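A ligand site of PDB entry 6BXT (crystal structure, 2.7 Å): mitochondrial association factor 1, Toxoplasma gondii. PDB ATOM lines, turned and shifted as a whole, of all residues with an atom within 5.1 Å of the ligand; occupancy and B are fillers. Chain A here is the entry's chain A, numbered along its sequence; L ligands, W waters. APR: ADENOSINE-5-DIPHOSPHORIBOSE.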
ATOM      1  N   PHE A  33      15.588 -10.469  33.480  1.00  0.00           N
ATOM      2  CA  PHE A  33      15.568 -11.603  32.567  1.00  0.00           C
ATOM      3  C   PHE A  33      16.316 -12.806  33.139  1.00  0.00           C
ATOM      4  O   PHE A  33      17.298 -12.665  33.861  1.00  0.00           O
ATOM      5  CB  PHE A  33      16.200 -11.226  31.223  1.00  0.00           C
ATOM      6  CG  PHE A  33      15.449 -10.155  30.471  1.00  0.00           C
ATOM      7  CD1 PHE A  33      14.059 -10.161  30.433  1.00  0.00           C
ATOM      8  CD2 PHE A  33      16.131  -9.157  29.812  1.00  0.00           C
ATOM      9  CE1 PHE A  33      13.376  -9.180  29.739  1.00  0.00           C
ATOM     10  CE2 PHE A  33      15.445  -8.167  29.116  1.00  0.00           C
ATOM     11  CZ  PHE A  33      14.071  -8.187  29.082  1.00  0.00           C
ATOM     12  N   THR A  34      15.818 -13.994  32.804  1.00  0.00           N
ATOM     13  CA  THR A  34      16.481 -15.242  33.184  1.00  0.00           C
ATOM     14  C   THR A  34      17.729 -15.427  32.321  1.00  0.00           C
ATOM     15  O   THR A  34      17.731 -15.061  31.148  1.00  0.00           O
ATOM     16  CB  THR A  34      15.523 -16.450  33.005  1.00  0.00           C
ATOM     17  OG1 THR A  34      14.342 -16.247  33.775  1.00  0.00           O
ATOM     18  CG2 THR A  34      16.187 -17.755  33.413  1.00  0.00           C
ATOM     19  N   LEU A  36      20.288 -17.196  29.837  1.00  0.00           N
ATOM     20  CA  LEU A  36      20.109 -18.169  28.764  1.00  0.00           C
ATOM     21  C   LEU A  36      20.485 -19.572  29.233  1.00  0.00           C
ATOM     22  O   LEU A  36      19.737 -20.526  29.020  1.00  0.00           O
ATOM     23  CB  LEU A  36      20.955 -17.778  27.545  1.00  0.00           C
ATOM     24  CG  LEU A  36      20.288 -16.946  26.447  1.00  0.00           C
ATOM     25  CD1 LEU A  36      19.421 -15.831  27.006  1.00  0.00           C
ATOM     26  CD2 LEU A  36      21.358 -16.374  25.521  1.00  0.00           C
ATOM     27  N   ALA A  50      14.635 -16.398  20.343  1.00  0.00           N
ATOM     28  CA  ALA A  50      13.540 -15.693  19.706  1.00  0.00           C
ATOM     29  C   ALA A  50      14.041 -15.048  18.420  1.00  0.00           C
ATOM     30  O   ALA A  50      14.411 -13.869  18.406  1.00  0.00           O
ATOM     31  CB  ALA A  50      12.957 -14.651  20.636  1.00  0.00           C
ATOM     32  N   GLY A  51      14.068 -15.838  17.345  1.00  0.00           N
ATOM     33  CA  GLY A  51      14.678 -15.420  16.094  1.00  0.00           C
ATOM     34  C   GLY A  51      13.895 -14.390  15.314  1.00  0.00           C
ATOM     35  O   GLY A  51      12.816 -13.960  15.728  1.00  0.00           O
ATOM     36  N   THR A  52      14.445 -14.009  14.161  1.00  0.00           N
ATOM     37  CA  THR A  52      13.846 -12.991  13.306  1.00  0.00           C
ATOM     38  C   THR A  52      13.580 -13.563  11.910  1.00  0.00           C
ATOM     39  O   THR A  52      13.921 -14.710  11.619  1.00  0.00           O
ATOM     40  CB  THR A  52      14.753 -11.750  13.182  1.00  0.00           C
ATOM     41  OG1 THR A  52      14.220 -10.858  12.197  1.00  0.00           O
ATOM     42  CG2 THR A  52      16.168 -12.164  12.785  1.00  0.00           C
ATOM     43  N   GLY A  58      21.789 -12.471  15.952  1.00  0.00           N
ATOM     44  CA  GLY A  58      22.327 -11.162  16.238  1.00  0.00           C
ATOM     45  C   GLY A  58      21.225 -10.173  16.551  1.00  0.00           C
ATOM     46  O   GLY A  58      20.162 -10.557  17.030  1.00  0.00           O
ATOM     47  N   GLY A  59      21.488  -8.903  16.271  1.00  0.00           N
ATOM     48  CA  GLY A  59      20.511  -7.859  16.541  1.00  0.00           C
ATOM     49  C   GLY A  59      20.428  -7.554  18.021  1.00  0.00           C
ATOM     50  O   GLY A  59      21.451  -7.518  18.711  1.00  0.00           O
ATOM     51  N   VAL A  60      19.210  -7.350  18.509  1.00  0.00           N
ATOM     52  CA  VAL A  60      18.973  -6.993  19.904  1.00  0.00           C
ATOM     53  C   VAL A  60      18.024  -7.992  20.551  1.00  0.00           C
ATOM     54  O   VAL A  60      17.875  -9.109  20.067  1.00  0.00           O
ATOM     55  CB  VAL A  60      18.401  -5.562  20.020  1.00  0.00           C
ATOM     56  CG1 VAL A  60      19.376  -4.557  19.433  1.00  0.00           C
ATOM     57  CG2 VAL A  60      17.034  -5.475  19.344  1.00  0.00           C
ATOM     58  N   GLY A  61      17.395  -7.587  21.660  1.00  0.00           N
ATOM     59  CA  GLY A  61      16.480  -8.465  22.373  1.00  0.00           C
ATOM     60  C   GLY A  61      17.188  -9.717  22.836  1.00  0.00           C
ATOM     61  O   GLY A  61      18.350  -9.670  23.246  1.00  0.00           O
ATOM     62  N   MET A  62      16.483 -10.842  22.771  1.00  0.00           N
ATOM     63  CA  MET A  62      17.043 -12.115  23.193  1.00  0.00           C
ATOM     64  C   MET A  62      17.972 -12.707  22.133  1.00  0.00           C
ATOM     65  O   MET A  62      18.892 -13.460  22.454  1.00  0.00           O
ATOM     66  CB  MET A  62      15.923 -13.110  23.509  1.00  0.00           C
ATOM     67  CG  MET A  62      16.425 -14.488  23.871  1.00  0.00           C
ATOM     68  SD  MET A  62      15.337 -15.348  25.003  1.00  0.00           S
ATOM     69  CE  MET A  62      16.205 -16.908  25.128  1.00  0.00           C
ATOM     70  N   ASN A  63      17.728 -12.368  20.871  1.00  0.00           N
ATOM     71  CA  ASN A  63      18.586 -12.815  19.789  1.00  0.00           C
ATOM     72  C   ASN A  63      19.971 -12.198  19.918  1.00  0.00           C
ATOM     73  O   ASN A  63      20.975 -12.789  19.505  1.00  0.00           O
ATOM     74  CB  ASN A  63      17.965 -12.466  18.430  1.00  0.00           C
ATOM     75  CG  ASN A  63      18.600 -13.205  17.268  1.00  0.00           C
ATOM     76  OD1 ASN A  63      19.324 -14.187  17.469  1.00  0.00           O
ATOM     77  ND2 ASN A  63      18.326 -12.753  16.056  1.00  0.00           N
ATOM     78  N   GLY A  64      20.026 -11.006  20.508  1.00  0.00           N
ATOM     79  CA  GLY A  64      21.288 -10.323  20.747  1.00  0.00           C
ATOM     80  C   GLY A  64      22.094 -10.994  21.843  1.00  0.00           C
ATOM     81  O   GLY A  64      23.320 -11.009  21.788  1.00  0.00           O
ATOM     82  N   GLU A  65      21.406 -11.541  22.833  1.00  0.00           N
ATOM     83  CA  GLU A  65      22.070 -12.228  23.939  1.00  0.00           C
ATOM     84  C   GLU A  65      22.825 -13.461  23.452  1.00  0.00           C
ATOM     85  O   GLU A  65      23.986 -13.662  23.813  1.00  0.00           O
ATOM     86  CB  GLU A  65      21.055 -12.650  25.005  1.00  0.00           C
ATOM     87  CG  GLU A  65      20.701 -11.544  25.980  1.00  0.00           C
ATOM     88  CD  GLU A  65      21.900 -11.059  26.776  1.00  0.00           C
ATOM     89  OE1 GLU A  65      22.541 -11.880  27.463  1.00  0.00           O
ATOM     90  OE2 GLU A  65      22.198  -9.846  26.701  1.00  0.00           O
ATOM     91  N   ALA A 172       8.893 -16.066  15.610  1.00  0.00           N
ATOM     92  CA  ALA A 172       7.543 -15.932  16.135  1.00  0.00           C
ATOM     93  C   ALA A 172       6.703 -14.996  15.260  1.00  0.00           C
ATOM     94  O   ALA A 172       7.247 -14.151  14.549  1.00  0.00           O
ATOM     95  CB  ALA A 172       7.588 -15.418  17.566  1.00  0.00           C
ATOM     96  N   PRO A 217      11.574 -18.292  26.054  1.00  0.00           N
ATOM     97  CA  PRO A 217      11.050 -16.959  26.377  1.00  0.00           C
ATOM     98  C   PRO A 217       9.579 -16.888  25.992  1.00  0.00           C
ATOM     99  O   PRO A 217       9.078 -17.843  25.406  1.00  0.00           O
ATOM    100  CB  PRO A 217      11.900 -16.038  25.516  1.00  0.00           C
ATOM    101  CG  PRO A 217      12.265 -16.868  24.339  1.00  0.00           C
ATOM    102  CD  PRO A 217      12.424 -18.269  24.856  1.00  0.00           C
ATOM    103  N   LEU A 218       8.910 -15.793  26.321  1.00  0.00           N
ATOM    104  CA  LEU A 218       7.543 -15.592  25.840  1.00  0.00           C
ATOM    105  C   LEU A 218       7.625 -15.090  24.402  1.00  0.00           C
ATOM    106  O   LEU A 218       7.780 -13.889  24.168  1.00  0.00           O
ATOM    107  CB  LEU A 218       6.782 -14.608  26.720  1.00  0.00           C
ATOM    108  CG  LEU A 218       5.303 -14.426  26.385  1.00  0.00           C
ATOM    109  CD1 LEU A 218       4.511 -15.698  26.672  1.00  0.00           C
ATOM    110  CD2 LEU A 218       4.720 -13.257  27.149  1.00  0.00           C
ATOM    111  N   LEU A 219       7.543 -16.016  23.446  1.00  0.00           N
ATOM    112  CA  LEU A 219       7.705 -15.688  22.028  1.00  0.00           C
ATOM    113  C   LEU A 219       6.758 -14.573  21.584  1.00  0.00           C
ATOM    114  O   LEU A 219       5.583 -14.559  21.941  1.00  0.00           O
ATOM    115  CB  LEU A 219       7.493 -16.934  21.157  1.00  0.00           C
ATOM    116  CG  LEU A 219       8.619 -17.971  20.984  1.00  0.00           C
ATOM    117  CD1 LEU A 219      10.007 -17.345  20.996  1.00  0.00           C
ATOM    118  CD2 LEU A 219       8.513 -19.088  22.029  1.00  0.00           C
ATOM    119  N   GLY A 220       7.287 -13.644  20.804  1.00  0.00           N
ATOM    120  CA  GLY A 220       6.487 -12.591  20.197  1.00  0.00           C
ATOM    121  C   GLY A 220       6.004 -11.540  21.183  1.00  0.00           C
ATOM    122  O   GLY A 220       5.069 -10.799  20.876  1.00  0.00           O
ATOM    123  N   ALA A 221       6.652 -11.464  22.344  1.00  0.00           N
ATOM    124  CA  ALA A 221       6.238 -10.537  23.388  1.00  0.00           C
ATOM    125  C   ALA A 221       7.189  -9.353  23.532  1.00  0.00           C
ATOM    126  O   ALA A 221       6.990  -8.485  24.378  1.00  0.00           O
ATOM    127  CB  ALA A 221       6.118 -11.262  24.719  1.00  0.00           C
ATOM    128  N   GLY A 222       8.219  -9.312  22.690  1.00  0.00           N
ATOM    129  CA  GLY A 222       9.185  -8.228  22.708  1.00  0.00           C
ATOM    130  C   GLY A 222       8.919  -7.233  21.598  1.00  0.00           C
ATOM    131  O   GLY A 222       7.945  -6.487  21.647  1.00  0.00           O
ATOM    132  N   HIS A 223       9.788  -7.225  20.583  1.00  0.00           N
ATOM    133  CA  HIS A 223       9.658  -6.293  19.467  1.00  0.00           C
ATOM    134  C   HIS A 223       8.589  -6.741  18.457  1.00  0.00           C
ATOM    135  O   HIS A 223       8.134  -5.922  17.649  1.00  0.00           O
ATOM    136  CB  HIS A 223      10.998  -6.113  18.750  1.00  0.00           C
ATOM    137  CG  HIS A 223      12.101  -5.595  19.622  1.00  0.00           C
ATOM    138  ND1 HIS A 223      12.900  -6.413  20.387  1.00  0.00           N
ATOM    139  CD2 HIS A 223      12.530  -4.331  19.852  1.00  0.00           C
ATOM    140  CE1 HIS A 223      13.777  -5.677  21.041  1.00  0.00           C
ATOM    141  NE2 HIS A 223      13.574  -4.417  20.737  1.00  0.00           N
ATOM    142  N   PHE A 224       8.210  -8.017  18.491  1.00  0.00           N
ATOM    143  CA  PHE A 224       7.154  -8.523  17.603  1.00  0.00           C
ATOM    144  C   PHE A 224       5.762  -8.326  18.204  1.00  0.00           C
ATOM    145  O   PHE A 224       4.777  -8.842  17.673  1.00  0.00           O
ATOM    146  CB  PHE A 224       7.350 -10.014  17.298  1.00  0.00           C
ATOM    147  CG  PHE A 224       8.461 -10.313  16.329  1.00  0.00           C
ATOM    148  CD1 PHE A 224       9.212  -9.300  15.747  1.00  0.00           C
ATOM    149  CD2 PHE A 224       8.731 -11.626  15.976  1.00  0.00           C
ATOM    150  CE1 PHE A 224      10.228  -9.599  14.854  1.00  0.00           C
ATOM    151  CE2 PHE A 224       9.746 -11.929  15.074  1.00  0.00           C
ATOM    152  CZ  PHE A 224      10.488 -10.912  14.512  1.00  0.00           C
ATOM    153  N   ARG A 225       5.660  -7.588  19.307  1.00  0.00           N
ATOM    154  CA  ARG A 225       4.371  -7.394  19.958  1.00  0.00           C
ATOM    155  C   ARG A 225       3.472  -6.446  19.156  1.00  0.00           C
ATOM    156  O   ARG A 225       2.279  -6.674  19.024  1.00  0.00           O
ATOM    157  CB  ARG A 225       4.548  -6.840  21.362  1.00  0.00           C
ATOM    158  CG  ARG A 225       3.298  -7.008  22.230  1.00  0.00           C
ATOM    159  CD  ARG A 225       3.230  -5.981  23.337  1.00  0.00           C
ATOM    160  NE  ARG A 225       4.407  -6.023  24.204  1.00  0.00           N
ATOM    161  CZ  ARG A 225       4.506  -5.364  25.357  1.00  0.00           C
ATOM    162  NH1 ARG A 225       5.609  -5.466  26.077  1.00  0.00           N
ATOM    163  NH2 ARG A 225       3.500  -4.625  25.787  1.00  0.00           N
ATOM    164  N   MET A 257      11.064 -18.475  30.792  1.00  0.00           N
ATOM    165  CA  MET A 257      11.869 -17.380  31.294  1.00  0.00           C
ATOM    166  C   MET A 257      10.985 -16.256  31.830  1.00  0.00           C
ATOM    167  O   MET A 257       9.783 -16.219  31.563  1.00  0.00           O
ATOM    168  CB  MET A 257      12.781 -16.850  30.198  1.00  0.00           C
ATOM    169  CG  MET A 257      13.736 -17.884  29.621  1.00  0.00           C
ATOM    170  SD  MET A 257      14.631 -17.271  28.195  1.00  0.00           S
ATOM    171  CE  MET A 257      15.624 -15.972  28.931  1.00  0.00           C
ATOM    172  N   GLU A 259       9.500 -12.438  32.454  1.00  0.00           N
ATOM    173  CA  GLU A 259       9.258 -11.086  31.987  1.00  0.00           C
ATOM    174  C   GLU A 259       8.208 -10.467  32.916  1.00  0.00           C
ATOM    175  O   GLU A 259       7.369 -11.191  33.463  1.00  0.00           O
ATOM    176  CB  GLU A 259       8.805 -11.073  30.519  1.00  0.00           C
ATOM    177  CG  GLU A 259       7.654 -12.009  30.188  1.00  0.00           C
ATOM    178  CD  GLU A 259       6.306 -11.465  30.605  1.00  0.00           C
ATOM    179  OE1 GLU A 259       6.164 -10.229  30.695  1.00  0.00           O
ATOM    180  OE2 GLU A 259       5.395 -12.284  30.849  1.00  0.00           O
HETATM  181  N1  APR L   1      17.318 -11.646  27.608  1.00  0.00           N
HETATM  182  C2  APR L   1      16.306 -12.470  27.961  1.00  0.00           C
HETATM  183  N3  APR L   1      15.013 -12.149  27.608  1.00  0.00           N
HETATM  184  C4  APR L   1      14.757 -11.010  26.924  1.00  0.00           C
HETATM  185  C5  APR L   1      15.769 -10.187  26.572  1.00  0.00           C
HETATM  186  C6  APR L   1      17.072 -10.505  26.923  1.00  0.00           C
HETATM  187  N6  APR L   1      18.342  -9.896  26.724  1.00  0.00           N
HETATM  188  N7  APR L   1      15.242  -9.124  25.889  1.00  0.00           N
HETATM  189  C8  APR L   1      13.902  -9.296  25.828  1.00  0.00           C
HETATM  190  N9  APR L   1      13.580 -10.468  26.467  1.00  0.00           N
HETATM  191  C1' APR L   1      12.334 -11.032  26.641  1.00  0.00           C
HETATM  192  C2' APR L   1      11.281 -10.262  26.318  1.00  0.00           C
HETATM  193  O2' APR L   1      10.671  -9.736  27.546  1.00  0.00           O
HETATM  194  C3' APR L   1      10.282 -11.202  25.606  1.00  0.00           C
HETATM  195  O3' APR L   1       9.368 -11.662  26.461  1.00  0.00           O
HETATM  196  O4' APR L   1      12.269 -12.398  25.708  1.00  0.00           O
HETATM  197  C4' APR L   1      11.177 -12.380  25.024  1.00  0.00           C
HETATM  198  C5' APR L   1      11.500 -12.137  23.575  1.00  0.00           C
HETATM  199  O5' APR L   1      12.335 -10.962  23.464  1.00  0.00           O
HETATM  200  PA  APR L   1      12.544 -10.354  22.040  1.00  0.00           P
HETATM  201  O1A APR L   1      13.530 -11.205  21.259  1.00  0.00           O
HETATM  202  O2A APR L   1      13.044  -8.972  22.137  1.00  0.00           O
HETATM  203  O3A APR L   1      11.112 -10.351  21.309  1.00  0.00           O
HETATM  204  PB  APR L   1      10.771 -11.050  19.914  1.00  0.00           P
HETATM  205  O1B APR L   1      10.550 -12.553  20.108  1.00  0.00           O
HETATM  206  O2B APR L   1       9.496 -10.402  19.374  1.00  0.00           O
HETATM  207  O5D APR L   1      11.952 -10.800  18.886  1.00  0.00           O
HETATM  208  C5D APR L   1      11.870  -9.586  18.173  1.00  0.00           C
HETATM  209  O4D APR L   1      14.070  -9.119  18.733  1.00  0.00           O
HETATM  210  O1D APR L   1      15.599 -10.894  19.408  1.00  0.00           O
HETATM  211  C1D APR L   1      15.377 -10.001  18.381  1.00  0.00           C
HETATM  212  O2D APR L   1      16.300 -10.376  16.288  1.00  0.00           O
HETATM  213  C2D APR L   1      15.158 -10.646  17.237  1.00  0.00           C
HETATM  214  O3D APR L   1      14.165  -9.428  15.504  1.00  0.00           O
HETATM  215  C3D APR L   1      13.891 -10.110  16.649  1.00  0.00           C
HETATM  216  C4D APR L   1      13.291  -9.120  17.721  1.00  0.00           C
HETATM  217  O   HOH W   1      12.834  -6.915  23.712  1.00  0.00           O
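The backbone NH (N) of Phe 224 is in hydrogen-bond range of an oxygen (O2B) of the ligand (2.8 Å). O of Val 60 is in hydrogen-bond range of O1D of the ligand (3.0 Å). The backbone NH (N) of Asn 63 sits at hydrogen-bond distance from an oxygen (O1D) of the ligand, 3.0 Å away. The side-chain amide nitrogen of Asn 63 sits at hydrogen-bond distance from an oxygen (O2D) of the ligand, at 3.1 Å. An oxygen (O2B) of the ligand lies within hydrogen-bond range of the backbone NH (N) of His 223 (3.4 Å). ND1 of His 223 lies within hydrogen-bond range of O2A of the ligand. The backbone NH (N) of Gly 222 sits close to an oxygen (O3A) of the ligand, at 3.4 Å. O1D of the ligand is in hydrogen-bond range of O of Ala 50. N of Met 62 sits at hydrogen-bond distance from O1A of the ligand. A nitrogen (N6) of the ligand sits at hydrogen-bond distance from the backbone carbonyl oxygen (O) of Gly 61, at 3.5 Å.
The side-chain amide nitrogen of Asn 63 sits at hydrogen-bond distance from the backbone carbonyl oxygen of Gly 58 (3.0 Å).
CE2 of Phe 33 touches C5 of the ligand, 3.3 Å away. Thr 52 touches the ligand (CB to O3D, 3.3 Å). Gly 58 touches the ligand. Glu 65 touches the ligand. Pro 217 touches the ligand (CB to O4', 3.7 Å). Leu 218 touches the ligand (O to O3', 3.6 Å). Gly 220 touches the ligand (N to O1B, 3.5 Å). Ala 221 touches the ligand. Met 257 touches the ligand (CE to C2, 3.7 Å). Glu 259 touches the ligand (CB to O2', 3.8 Å). Hydrophobic or aromatic side chains within 4 Å of the ligand: Phe 33, Ala 50, Met 62, Pro 217, Leu 218, Ala 221, His 223, Phe 224 and Met 257. Within 4 Å of the ligand: Phe 33, Ala 50, Thr 52, Gly 58, Val 60, Gly 61, Met 62, Asn 63, Glu 65, Pro 217, Leu 218, Gly 220, Ala 221, Gly 222, His 223, Phe 224, Met 257 and Glu 259. The nearest printed residue that does not touch the ligand is Gly 51 (4.1 Å).
Water W1 bridges O2A of the ligand (2.6 Å) and ND1 of His 223 (3.4 Å).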
